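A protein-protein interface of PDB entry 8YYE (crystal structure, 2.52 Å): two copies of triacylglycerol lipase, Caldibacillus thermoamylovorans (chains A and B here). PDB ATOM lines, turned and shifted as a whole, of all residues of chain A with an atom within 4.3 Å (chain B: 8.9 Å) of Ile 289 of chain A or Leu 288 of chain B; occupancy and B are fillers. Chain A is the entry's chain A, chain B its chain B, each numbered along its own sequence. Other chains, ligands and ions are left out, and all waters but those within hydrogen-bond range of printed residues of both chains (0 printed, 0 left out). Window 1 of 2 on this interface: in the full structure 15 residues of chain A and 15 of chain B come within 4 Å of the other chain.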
ATOM      1  N   PHE A 169      26.962 -31.284  13.886  1.00  0.00           N
ATOM      2  CA  PHE A 169      26.150 -30.076  13.994  1.00  0.00           C
ATOM      3  C   PHE A 169      26.981 -28.832  13.696  1.00  0.00           C
ATOM      4  O   PHE A 169      26.631 -28.047  12.804  1.00  0.00           O
ATOM      5  CB  PHE A 169      25.508 -29.977  15.382  1.00  0.00           C
ATOM      6  CG  PHE A 169      24.681 -28.740  15.585  1.00  0.00           C
ATOM      7  CD1 PHE A 169      23.683 -28.390  14.673  1.00  0.00           C
ATOM      8  CD2 PHE A 169      24.850 -27.956  16.709  1.00  0.00           C
ATOM      9  CE1 PHE A 169      22.886 -27.254  14.867  1.00  0.00           C
ATOM     10  CE2 PHE A 169      24.061 -26.820  16.910  1.00  0.00           C
ATOM     11  CZ  PHE A 169      23.080 -26.472  15.994  1.00  0.00           C
ATOM     12  N   PHE A 178      22.645 -21.535  17.573  1.00  0.00           N
ATOM     13  CA  PHE A 178      22.539 -22.447  18.714  1.00  0.00           C
ATOM     14  C   PHE A 178      22.734 -21.713  20.035  1.00  0.00           C
ATOM     15  O   PHE A 178      22.025 -21.981  21.006  1.00  0.00           O
ATOM     16  CB  PHE A 178      23.544 -23.594  18.599  1.00  0.00           C
ATOM     17  CG  PHE A 178      23.713 -24.392  19.885  1.00  0.00           C
ATOM     18  CD1 PHE A 178      22.735 -25.287  20.306  1.00  0.00           C
ATOM     19  CD2 PHE A 178      24.865 -24.265  20.662  1.00  0.00           C
ATOM     20  CE1 PHE A 178      22.894 -26.024  21.487  1.00  0.00           C
ATOM     21  CE2 PHE A 178      25.023 -24.998  21.847  1.00  0.00           C
ATOM     22  CZ  PHE A 178      24.029 -25.881  22.252  1.00  0.00           C
ATOM     23  N   LEU A 285      16.164 -28.663  23.686  1.00  0.00           N
ATOM     24  CA  LEU A 285      17.146 -27.841  22.973  1.00  0.00           C
ATOM     25  C   LEU A 285      17.946 -28.656  21.960  1.00  0.00           C
ATOM     26  O   LEU A 285      18.436 -28.104  20.968  1.00  0.00           O
ATOM     27  CB  LEU A 285      18.087 -27.160  23.972  1.00  0.00           C
ATOM     28  CG  LEU A 285      19.376 -26.493  23.476  1.00  0.00           C
ATOM     29  CD1 LEU A 285      19.142 -25.155  22.774  1.00  0.00           C
ATOM     30  CD2 LEU A 285      20.352 -26.312  24.617  1.00  0.00           C
ATOM     31  N   PHE A 286      18.074 -29.969  22.176  1.00  0.00           N
ATOM     32  CA  PHE A 286      18.883 -30.807  21.308  1.00  0.00           C
ATOM     33  C   PHE A 286      18.080 -31.766  20.435  1.00  0.00           C
ATOM     34  O   PHE A 286      18.680 -32.449  19.605  1.00  0.00           O
ATOM     35  CB  PHE A 286      19.883 -31.591  22.146  1.00  0.00           C
ATOM     36  CG  PHE A 286      20.834 -30.713  22.905  1.00  0.00           C
ATOM     37  CD1 PHE A 286      21.891 -30.100  22.263  1.00  0.00           C
ATOM     38  CD2 PHE A 286      20.663 -30.491  24.262  1.00  0.00           C
ATOM     39  CE1 PHE A 286      22.759 -29.290  22.957  1.00  0.00           C
ATOM     40  CE2 PHE A 286      21.537 -29.680  24.962  1.00  0.00           C
ATOM     41  CZ  PHE A 286      22.583 -29.080  24.310  1.00  0.00           C
ATOM     42  N   THR A 287      16.747 -31.831  20.590  1.00  0.00           N
ATOM     43  CA  THR A 287      15.916 -32.786  19.845  1.00  0.00           C
ATOM     44  C   THR A 287      16.198 -32.746  18.351  1.00  0.00           C
ATOM     45  O   THR A 287      16.470 -33.776  17.721  1.00  0.00           O
ATOM     46  CB  THR A 287      14.430 -32.492  20.077  1.00  0.00           C
ATOM     47  OG1 THR A 287      14.149 -32.549  21.474  1.00  0.00           O
ATOM     48  CG2 THR A 287      13.578 -33.471  19.331  1.00  0.00           C
ATOM     49  N   LEU A 288      16.060 -31.566  17.758  1.00  0.00           N
ATOM     50  CA  LEU A 288      16.205 -31.430  16.313  1.00  0.00           C
ATOM     51  C   LEU A 288      17.665 -31.545  15.877  1.00  0.00           C
ATOM     52  O   LEU A 288      17.959 -32.189  14.860  1.00  0.00           O
ATOM     53  CB  LEU A 288      15.602 -30.097  15.874  1.00  0.00           C
ATOM     54  CG  LEU A 288      14.099 -29.938  16.099  1.00  0.00           C
ATOM     55  CD1 LEU A 288      13.528 -29.017  15.057  1.00  0.00           C
ATOM     56  CD2 LEU A 288      13.379 -31.291  16.022  1.00  0.00           C
ATOM     57  N   ILE A 289      18.592 -30.919  16.618  1.00  0.00           N
ATOM     58  CA  ILE A 289      20.014 -31.130  16.342  1.00  0.00           C
ATOM     59  C   ILE A 289      20.335 -32.621  16.282  1.00  0.00           C
ATOM     60  O   ILE A 289      21.027 -33.091  15.365  1.00  0.00           O
ATOM     61  CB  ILE A 289      20.888 -30.421  17.391  1.00  0.00           C
ATOM     62  CG1 ILE A 289      20.755 -28.895  17.253  1.00  0.00           C
ATOM     63  CG2 ILE A 289      22.344 -30.906  17.253  1.00  0.00           C
ATOM     64  CD1 ILE A 289      21.194 -28.124  18.456  1.00  0.00           C
ATOM     65  N   SER A 290      19.819 -33.392  17.248  1.00  0.00           N
ATOM     66  CA  SER A 290      20.090 -34.821  17.258  1.00  0.00           C
ATOM     67  C   SER A 290      19.520 -35.480  16.005  1.00  0.00           C
ATOM     68  O   SER A 290      20.172 -36.331  15.387  1.00  0.00           O
ATOM     69  CB  SER A 290      19.533 -35.446  18.536  1.00  0.00           C
ATOM     70  OG  SER A 290      20.044 -36.752  18.710  1.00  0.00           O
ATOM     71  N   MET A 291      18.337 -35.036  15.569  1.00  0.00           N
ATOM     72  CA  MET A 291      17.725 -35.588  14.362  1.00  0.00           C
ATOM     73  C   MET A 291      18.579 -35.314  13.123  1.00  0.00           C
ATOM     74  O   MET A 291      18.766 -36.203  12.284  1.00  0.00           O
ATOM     75  CB  MET A 291      16.313 -35.029  14.184  1.00  0.00           C
ATOM     76  CG  MET A 291      15.224 -35.931  14.708  1.00  0.00           C
ATOM     77  SD  MET A 291      14.568 -37.028  13.439  1.00  0.00           S
ATOM     78  CE  MET A 291      13.218 -36.026  12.770  1.00  0.00           C
ATOM     79  N   GLN A 292      19.093 -34.084  12.963  1.00  0.00           N
ATOM     80  CA  GLN A 292      19.937 -33.859  11.787  1.00  0.00           C
ATOM     81  C   GLN A 292      21.253 -34.619  11.907  1.00  0.00           C
ATOM     82  O   GLN A 292      21.719 -35.207  10.927  1.00  0.00           O
ATOM     83  CB  GLN A 292      20.179 -32.367  11.513  1.00  0.00           C
ATOM     84  CG  GLN A 292      20.880 -31.597  12.580  1.00  0.00           C
ATOM     85  CD  GLN A 292      22.373 -31.428  12.319  1.00  0.00           C
ATOM     86  OE1 GLN A 292      22.854 -31.551  11.181  1.00  0.00           O
ATOM     87  NE2 GLN A 292      23.129 -31.231  13.396  1.00  0.00           N
ATOM     88  N   MET A 293      21.839 -34.672  13.108  1.00  0.00           N
ATOM     89  CA  MET A 293      23.071 -35.445  13.279  1.00  0.00           C
ATOM     90  C   MET A 293      22.819 -36.930  13.047  1.00  0.00           C
ATOM     91  O   MET A 293      23.635 -37.617  12.424  1.00  0.00           O
ATOM     92  CB  MET A 293      23.663 -35.224  14.673  1.00  0.00           C
ATOM     93  CG  MET A 293      24.373 -33.883  14.825  1.00  0.00           C
ATOM     94  SD  MET A 293      24.973 -33.588  16.505  1.00  0.00           S
ATOM     95  CE  MET A 293      25.911 -35.078  16.752  1.00  0.00           C
ATOM     96  N   GLY A 314      23.030 -35.825  21.570  1.00  0.00           N
ATOM     97  CA  GLY A 314      22.341 -34.557  21.405  1.00  0.00           C
ATOM     98  C   GLY A 314      23.125 -33.526  20.582  1.00  0.00           C
ATOM     99  O   GLY A 314      22.518 -32.793  19.799  1.00  0.00           O
ATOM    100  N   PHE B 169       7.540 -29.619   7.882  1.00  0.00           N
ATOM    101  CA  PHE B 169       7.906 -29.837   9.277  1.00  0.00           C
ATOM    102  C   PHE B 169       6.889 -30.712   9.994  1.00  0.00           C
ATOM    103  O   PHE B 169       7.258 -31.716  10.620  1.00  0.00           O
ATOM    104  CB  PHE B 169       8.056 -28.521  10.025  1.00  0.00           C
ATOM    105  CG  PHE B 169       8.446 -28.716  11.451  1.00  0.00           C
ATOM    106  CD1 PHE B 169       9.581 -29.474  11.753  1.00  0.00           C
ATOM    107  CD2 PHE B 169       7.730 -28.140  12.478  1.00  0.00           C
ATOM    108  CE1 PHE B 169       9.988 -29.686  13.064  1.00  0.00           C
ATOM    109  CE2 PHE B 169       8.128 -28.332  13.801  1.00  0.00           C
ATOM    110  CZ  PHE B 169       9.263 -29.105  14.096  1.00  0.00           C
ATOM    111  N   GLN B 172       7.003 -34.547   9.939  1.00  0.00           N
ATOM    112  CA  GLN B 172       7.915 -35.399  10.703  1.00  0.00           C
ATOM    113  C   GLN B 172       7.440 -35.730  12.116  1.00  0.00           C
ATOM    114  O   GLN B 172       8.230 -36.271  12.892  1.00  0.00           O
ATOM    115  CB  GLN B 172       9.315 -34.781  10.791  1.00  0.00           C
ATOM    116  CG  GLN B 172      10.218 -35.151   9.623  1.00  0.00           C
ATOM    117  CD  GLN B 172       9.990 -34.241   8.440  1.00  0.00           C
ATOM    118  OE1 GLN B 172      10.136 -34.644   7.286  1.00  0.00           O
ATOM    119  NE2 GLN B 172       9.618 -33.000   8.723  1.00  0.00           N
ATOM    120  N   SER B 177       7.396 -31.982  20.507  1.00  0.00           N
ATOM    121  CA  SER B 177       8.675 -31.400  20.884  1.00  0.00           C
ATOM    122  C   SER B 177       8.720 -29.926  20.518  1.00  0.00           C
ATOM    123  O   SER B 177       9.239 -29.097  21.277  1.00  0.00           O
ATOM    124  CB  SER B 177       9.800 -32.176  20.207  1.00  0.00           C
ATOM    125  OG  SER B 177      11.034 -31.542  20.436  1.00  0.00           O
ATOM    126  N   ASP B 181       9.334 -26.732  23.207  1.00  0.00           N
ATOM    127  CA  ASP B 181      10.322 -25.684  22.970  1.00  0.00           C
ATOM    128  C   ASP B 181       9.676 -24.306  22.844  1.00  0.00           C
ATOM    129  O   ASP B 181      10.203 -23.313  23.363  1.00  0.00           O
ATOM    130  CB  ASP B 181      11.121 -26.011  21.714  1.00  0.00           C
ATOM    131  CG  ASP B 181      12.423 -25.271  21.658  1.00  0.00           C
ATOM    132  OD1 ASP B 181      12.775 -24.648  22.682  1.00  0.00           O
ATOM    133  OD2 ASP B 181      13.104 -25.319  20.612  1.00  0.00           O
ATOM    134  N   TYR B 276      17.924 -25.233   0.548  1.00  0.00           N
ATOM    135  CA  TYR B 276      17.659 -23.920   1.120  1.00  0.00           C
ATOM    136  C   TYR B 276      18.033 -23.904   2.600  1.00  0.00           C
ATOM    137  O   TYR B 276      17.748 -24.859   3.332  1.00  0.00           O
ATOM    138  CB  TYR B 276      16.198 -23.523   0.900  1.00  0.00           C
ATOM    139  CG  TYR B 276      15.984 -22.949  -0.481  1.00  0.00           C
ATOM    140  CD1 TYR B 276      15.944 -23.779  -1.601  1.00  0.00           C
ATOM    141  CD2 TYR B 276      15.861 -21.574  -0.679  1.00  0.00           C
ATOM    142  CE1 TYR B 276      15.765 -23.262  -2.882  1.00  0.00           C
ATOM    143  CE2 TYR B 276      15.679 -21.048  -1.954  1.00  0.00           C
ATOM    144  CZ  TYR B 276      15.634 -21.897  -3.052  1.00  0.00           C
ATOM    145  OH  TYR B 276      15.470 -21.379  -4.321  1.00  0.00           O
ATOM    146  N   TYR B 277      18.690 -22.827   3.031  1.00  0.00           N
ATOM    147  CA  TYR B 277      19.166 -22.688   4.399  1.00  0.00           C
ATOM    148  C   TYR B 277      18.594 -21.411   5.014  1.00  0.00           C
ATOM    149  O   TYR B 277      18.317 -20.441   4.293  1.00  0.00           O
ATOM    150  CB  TYR B 277      20.708 -22.678   4.441  1.00  0.00           C
ATOM    151  CG  TYR B 277      21.295 -23.904   3.750  1.00  0.00           C
ATOM    152  CD1 TYR B 277      21.549 -25.088   4.452  1.00  0.00           C
ATOM    153  CD2 TYR B 277      21.522 -23.897   2.373  1.00  0.00           C
ATOM    154  CE1 TYR B 277      22.041 -26.212   3.798  1.00  0.00           C
ATOM    155  CE2 TYR B 277      22.008 -25.016   1.713  1.00  0.00           C
ATOM    156  CZ  TYR B 277      22.267 -26.169   2.420  1.00  0.00           C
ATOM    157  OH  TYR B 277      22.750 -27.261   1.728  1.00  0.00           O
ATOM    158  N   PRO B 278      18.364 -21.394   6.331  1.00  0.00           N
ATOM    159  CA  PRO B 278      17.853 -20.173   6.966  1.00  0.00           C
ATOM    160  C   PRO B 278      18.836 -19.016   6.833  1.00  0.00           C
ATOM    161  O   PRO B 278      20.060 -19.203   6.837  1.00  0.00           O
ATOM    162  CB  PRO B 278      17.692 -20.582   8.433  1.00  0.00           C
ATOM    163  CG  PRO B 278      18.681 -21.682   8.633  1.00  0.00           C
ATOM    164  CD  PRO B 278      18.664 -22.442   7.324  1.00  0.00           C
ATOM    165  N   MET B 282      16.846 -15.190  11.035  1.00  0.00           N
ATOM    166  CA  MET B 282      15.789 -16.080  11.499  1.00  0.00           C
ATOM    167  C   MET B 282      15.842 -16.331  13.004  1.00  0.00           C
ATOM    168  O   MET B 282      16.905 -16.582  13.576  1.00  0.00           O
ATOM    169  CB  MET B 282      15.885 -17.406  10.775  1.00  0.00           C
ATOM    170  CG  MET B 282      14.926 -18.399  11.325  1.00  0.00           C
ATOM    171  SD  MET B 282      14.642 -19.802  10.287  1.00  0.00           S
ATOM    172  CE  MET B 282      14.090 -19.050   8.769  1.00  0.00           C
ATOM    173  N   HIS B 283      14.679 -16.290  13.633  1.00  0.00           N
ATOM    174  CA  HIS B 283      14.590 -16.672  15.028  1.00  0.00           C
ATOM    175  C   HIS B 283      15.182 -18.064  15.228  1.00  0.00           C
ATOM    176  O   HIS B 283      14.852 -19.004  14.491  1.00  0.00           O
ATOM    177  CB  HIS B 283      13.136 -16.660  15.495  1.00  0.00           C
ATOM    178  CG  HIS B 283      12.467 -15.311  15.413  1.00  0.00           C
ATOM    179  ND1 HIS B 283      12.204 -14.633  14.236  1.00  0.00           N
ATOM    180  CD2 HIS B 283      12.018 -14.518  16.419  1.00  0.00           C
ATOM    181  CE1 HIS B 283      11.611 -13.476  14.523  1.00  0.00           C
ATOM    182  NE2 HIS B 283      11.476 -13.397  15.833  1.00  0.00           N
ATOM    183  N   PRO B 284      16.047 -18.245  16.224  1.00  0.00           N
ATOM    184  CA  PRO B 284      16.694 -19.555  16.376  1.00  0.00           C
ATOM    185  C   PRO B 284      15.712 -20.671  16.691  1.00  0.00           C
ATOM    186  O   PRO B 284      16.036 -21.841  16.471  1.00  0.00           O
ATOM    187  CB  PRO B 284      17.695 -19.327  17.518  1.00  0.00           C
ATOM    188  CG  PRO B 284      17.188 -18.088  18.215  1.00  0.00           C
ATOM    189  CD  PRO B 284      16.568 -17.250  17.169  1.00  0.00           C
ATOM    190  N   LEU B 285      14.506 -20.355  17.157  1.00  0.00           N
ATOM    191  CA  LEU B 285      13.516 -21.412  17.334  1.00  0.00           C
ATOM    192  C   LEU B 285      13.254 -22.148  16.020  1.00  0.00           C
ATOM    193  O   LEU B 285      12.900 -23.330  16.044  1.00  0.00           O
ATOM    194  CB  LEU B 285      12.218 -20.843  17.935  1.00  0.00           C
ATOM    195  CG  LEU B 285      11.002 -21.782  18.057  1.00  0.00           C
ATOM    196  CD1 LEU B 285      11.203 -22.822  19.172  1.00  0.00           C
ATOM    197  CD2 LEU B 285       9.694 -21.021  18.288  1.00  0.00           C
ATOM    198  N   PHE B 286      13.488 -21.505  14.871  1.00  0.00           N
ATOM    199  CA  PHE B 286      13.199 -22.115  13.578  1.00  0.00           C
ATOM    200  C   PHE B 286      14.413 -22.533  12.762  1.00  0.00           C
ATOM    201  O   PHE B 286      14.238 -23.043  11.647  1.00  0.00           O
ATOM    202  CB  PHE B 286      12.350 -21.182  12.726  1.00  0.00           C
ATOM    203  CG  PHE B 286      11.034 -20.938  13.311  1.00  0.00           C
ATOM    204  CD1 PHE B 286      10.076 -21.939  13.298  1.00  0.00           C
ATOM    205  CD2 PHE B 286      10.727 -19.709  13.860  1.00  0.00           C
ATOM    206  CE1 PHE B 286       8.846 -21.723  13.851  1.00  0.00           C
ATOM    207  CE2 PHE B 286       9.473 -19.482  14.407  1.00  0.00           C
ATOM    208  CZ  PHE B 286       8.542 -20.492  14.410  1.00  0.00           C
ATOM    209  N   THR B 287      15.629 -22.351  13.274  1.00  0.00           N
ATOM    210  CA  THR B 287      16.813 -22.595  12.456  1.00  0.00           C
ATOM    211  C   THR B 287      16.883 -24.050  11.994  1.00  0.00           C
ATOM    212  O   THR B 287      17.141 -24.329  10.816  1.00  0.00           O
ATOM    213  CB  THR B 287      18.076 -22.193  13.233  1.00  0.00           C
ATOM    214  OG1 THR B 287      17.969 -20.814  13.626  1.00  0.00           O
ATOM    215  CG2 THR B 287      19.300 -22.349  12.372  1.00  0.00           C
ATOM    216  N   LEU B 288      16.650 -24.998  12.904  1.00  0.00           N
ATOM    217  CA  LEU B 288      16.790 -26.400  12.527  1.00  0.00           C
ATOM    218  C   LEU B 288      15.609 -26.852  11.673  1.00  0.00           C
ATOM    219  O   LEU B 288      15.782 -27.584  10.684  1.00  0.00           O
ATOM    220  CB  LEU B 288      16.907 -27.264  13.780  1.00  0.00           C
ATOM    221  CG  LEU B 288      18.336 -27.636  14.196  1.00  0.00           C
ATOM    222  CD1 LEU B 288      19.085 -28.310  13.053  1.00  0.00           C
ATOM    223  CD2 LEU B 288      19.085 -26.417  14.676  1.00  0.00           C
ATOM    224  N   ILE B 289      14.398 -26.423  12.039  1.00  0.00           N
ATOM    225  CA  ILE B 289      13.231 -26.708  11.222  1.00  0.00           C
ATOM    226  C   ILE B 289      13.474 -26.215   9.807  1.00  0.00           C
ATOM    227  O   ILE B 289      13.190 -26.915   8.824  1.00  0.00           O
ATOM    228  CB  ILE B 289      11.985 -26.063  11.848  1.00  0.00           C
ATOM    229  CG1 ILE B 289      11.764 -26.664  13.236  1.00  0.00           C
ATOM    230  CG2 ILE B 289      10.754 -26.300  10.968  1.00  0.00           C
ATOM    231  CD1 ILE B 289      10.876 -25.844  14.128  1.00  0.00           C
ATOM    232  N   SER B 290      14.050 -25.014   9.693  1.00  0.00           N
ATOM    233  CA  SER B 290      14.328 -24.460   8.373  1.00  0.00           C
ATOM    234  C   SER B 290      15.303 -25.348   7.612  1.00  0.00           C
ATOM    235  O   SER B 290      15.107 -25.640   6.422  1.00  0.00           O
ATOM    236  CB  SER B 290      14.875 -23.040   8.510  1.00  0.00           C
ATOM    237  OG  SER B 290      14.949 -22.436   7.233  1.00  0.00           O
ATOM    238  N   MET B 291      16.354 -25.810   8.292  1.00  0.00           N
ATOM    239  CA  MET B 291      17.360 -26.609   7.608  1.00  0.00           C
ATOM    240  C   MET B 291      16.745 -27.909   7.114  1.00  0.00           C
ATOM    241  O   MET B 291      16.975 -28.334   5.976  1.00  0.00           O
ATOM    242  CB  MET B 291      18.512 -26.893   8.549  1.00  0.00           C
ATOM    243  CG  MET B 291      19.560 -25.834   8.581  1.00  0.00           C
ATOM    244  SD  MET B 291      20.477 -26.081  10.107  1.00  0.00           S
ATOM    245  CE  MET B 291      20.861 -27.817   9.913  1.00  0.00           C
ATOM    246  N   GLN B 292      15.941 -28.549   7.964  1.00  0.00           N
ATOM    247  CA  GLN B 292      15.290 -29.783   7.557  1.00  0.00           C
ATOM    248  C   GLN B 292      14.352 -29.539   6.376  1.00  0.00           C
ATOM    249  O   GLN B 292      14.444 -30.221   5.351  1.00  0.00           O
ATOM    250  CB  GLN B 292      14.560 -30.380   8.759  1.00  0.00           C
ATOM    251  CG  GLN B 292      13.625 -31.502   8.445  1.00  0.00           C
ATOM    252  CD  GLN B 292      12.241 -31.011   8.128  1.00  0.00           C
ATOM    253  OE1 GLN B 292      11.665 -31.393   7.114  1.00  0.00           O
ATOM    254  NE2 GLN B 292      11.704 -30.135   8.976  1.00  0.00           N
ATOM    255  N   MET B 293      13.475 -28.535   6.478  1.00  0.00           N
ATOM    256  CA  MET B 293      12.532 -28.279   5.392  1.00  0.00           C
ATOM    257  C   MET B 293      13.247 -27.879   4.105  1.00  0.00           C
ATOM    258  O   MET B 293      12.791 -28.223   3.011  1.00  0.00           O
ATOM    259  CB  MET B 293      11.550 -27.178   5.788  1.00  0.00           C
ATOM    260  CG  MET B 293      10.512 -27.558   6.817  1.00  0.00           C
ATOM    261  SD  MET B 293       9.603 -26.080   7.315  1.00  0.00           S
ATOM    262  CE  MET B 293       8.635 -25.704   5.860  1.00  0.00           C
ATOM    263  N   GLY B 294      14.349 -27.131   4.213  1.00  0.00           N
ATOM    264  CA  GLY B 294      15.095 -26.703   3.042  1.00  0.00           C
ATOM    265  C   GLY B 294      15.814 -27.824   2.318  1.00  0.00           C
ATOM    266  O   GLY B 294      16.352 -27.598   1.230  1.00  0.00           O
ATOM    267  N   SER B 295      15.817 -29.034   2.884  1.00  0.00           N
ATOM    268  CA  SER B 295      16.443 -30.176   2.236  1.00  0.00           C
ATOM    269  C   SER B 295      15.540 -31.409   2.218  1.00  0.00           C
ATOM    270  O   SER B 295      16.043 -32.529   2.054  1.00  0.00           O
ATOM    271  CB  SER B 295      17.756 -30.493   2.930  1.00  0.00           C
ATOM    272  OG  SER B 295      17.493 -30.775   4.287  1.00  0.00           O
ATOM    273  N   ASN B 312      11.248 -21.613   2.569  1.00  0.00           N
ATOM    274  CA  ASN B 312      10.363 -21.568   3.720  1.00  0.00           C
ATOM    275  C   ASN B 312      10.663 -20.335   4.568  1.00  0.00           C
ATOM    276  O   ASN B 312      11.707 -19.683   4.420  1.00  0.00           O
ATOM    277  CB  ASN B 312      10.529 -22.825   4.556  1.00  0.00           C
ATOM    278  CG  ASN B 312      11.945 -22.976   5.067  1.00  0.00           C
ATOM    279  OD1 ASN B 312      12.238 -22.563   6.196  1.00  0.00           O
ATOM    280  ND2 ASN B 312      12.839 -23.508   4.230  1.00  0.00           N
ATOM    281  N   GLY B 314      10.810 -20.629   7.918  1.00  0.00           N
ATOM    282  CA  GLY B 314      11.157 -21.210   9.204  1.00  0.00           C
ATOM    283  C   GLY B 314      10.273 -22.390   9.606  1.00  0.00           C
ATOM    284  O   GLY B 314      10.756 -23.314  10.267  1.00  0.00           O
ATOM    285  N   ILE B 315       8.995 -22.353   9.221  1.00  0.00           N
ATOM    286  CA  ILE B 315       8.075 -23.434   9.572  1.00  0.00           C
ATOM    287  C   ILE B 315       7.016 -23.677   8.492  1.00  0.00           C
ATOM    288  O   ILE B 315       6.342 -24.712   8.508  1.00  0.00           O
ATOM    289  CB  ILE B 315       7.404 -23.171  10.936  1.00  0.00           C
ATOM    290  CG1 ILE B 315       6.837 -24.480  11.508  1.00  0.00           C
ATOM    291  CG2 ILE B 315       6.307 -22.144  10.813  1.00  0.00           C
ATOM    292  CD1 ILE B 315       6.854 -24.568  13.011  1.00  0.00           C
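Printed residues of chain B that touch a printed residue of chain A: Ser 177, Leu 288 and Ile 289. Hydrophobic or aromatic side chains of chain B within 4 Å of the printed part of chain A: Leu 288 and Ile 289. Among the printed residues, 6 pairs touch across the chains. Among the printed residues, no Asp or Glu carboxylate lies within 4 Å of a Lys or Arg side-chain nitrogen of the other chain.
CD2 of Leu 288 of chain B touches CE1 of Phe 169 of chain A, 3.9 Å away. Leu 288 of chain A touches Leu 288 of chain B (CB to CB, 3.8 Å). CD1 of Leu 288 of chain A touches CG1 of Ile 289 of chain B (3.5 Å). CG1 of Ile 289 of chain A touches CD2 of Leu 288 of chain B (3.9 Å). Gln 292 of chain A touches Leu 288 of chain B.
The backbone carbonyl oxygen (O) of Ile 289 of chain A lies close to the side-chain amide nitrogen (NE2) of Gln 292 of chain A (3.4 Å).
The side-chain hydroxyl (OG) of Ser 177 of chain B sits close to the side-chain hydroxyl (OG1) of Thr 287 of chain A (3.4 Å).
Phe 169 of chain A touches Leu 288 of chain B, but with the chains exchanged Leu 288 of chain A does not touch Phe 169 of chain B (4.1 Å). Leu 288 of chain A touches its own counterpart, Leu 288 of chain B. Leu 288 of chain A touches Ile 289 of chain B, and with the chains exchanged Ile 289 of chain A touches Leu 288 of chain B. Gln 292 of chain A touches Leu 288 of chain B, but with the chains exchanged Leu 288 of chain A does not touch Gln 292 of chain B (6.4 Å). Positions printed for both chains: 169, 285, 286, 287, 288, 289, 290, 291, 292, 293 and 314. Of the 6 pairs that touch across the chains among the printed residues, 3 have their exchanged pair printed and touching as well.
Of the printed residues of chain B, Phe 169 of chain A touches Leu 288 (3.9 Å). Printed residues of chain B within 4 Å of Thr 287 of chain A: Ser 177. Of the printed residues of chain B, Leu 288 of chain A touches Leu 288 and Ile 289. Of chain B, only Leu 288 comes within 4 Å of Ile 289 of chain A. No residue of chain B comes within 4 Å of Ser 290 of chain A. Printed residues of chain A within 4 Å of Ser 177 of chain B: Thr 287. Pro 284 of chain B touches none of the printed residues of chain A. Printed residues of chain A within 4 Å of Leu 288 of chain B: Phe 169, Leu 288, Ile 289 and Gln 292. The nearest residue of chain B that does not touch Ile 289 of chain A is Met 291 of chain B (7.3 Å). The nearest printed residue of chain A that does not touch Leu 288 of chain B is Leu 285 of chain A (6.5 Å).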
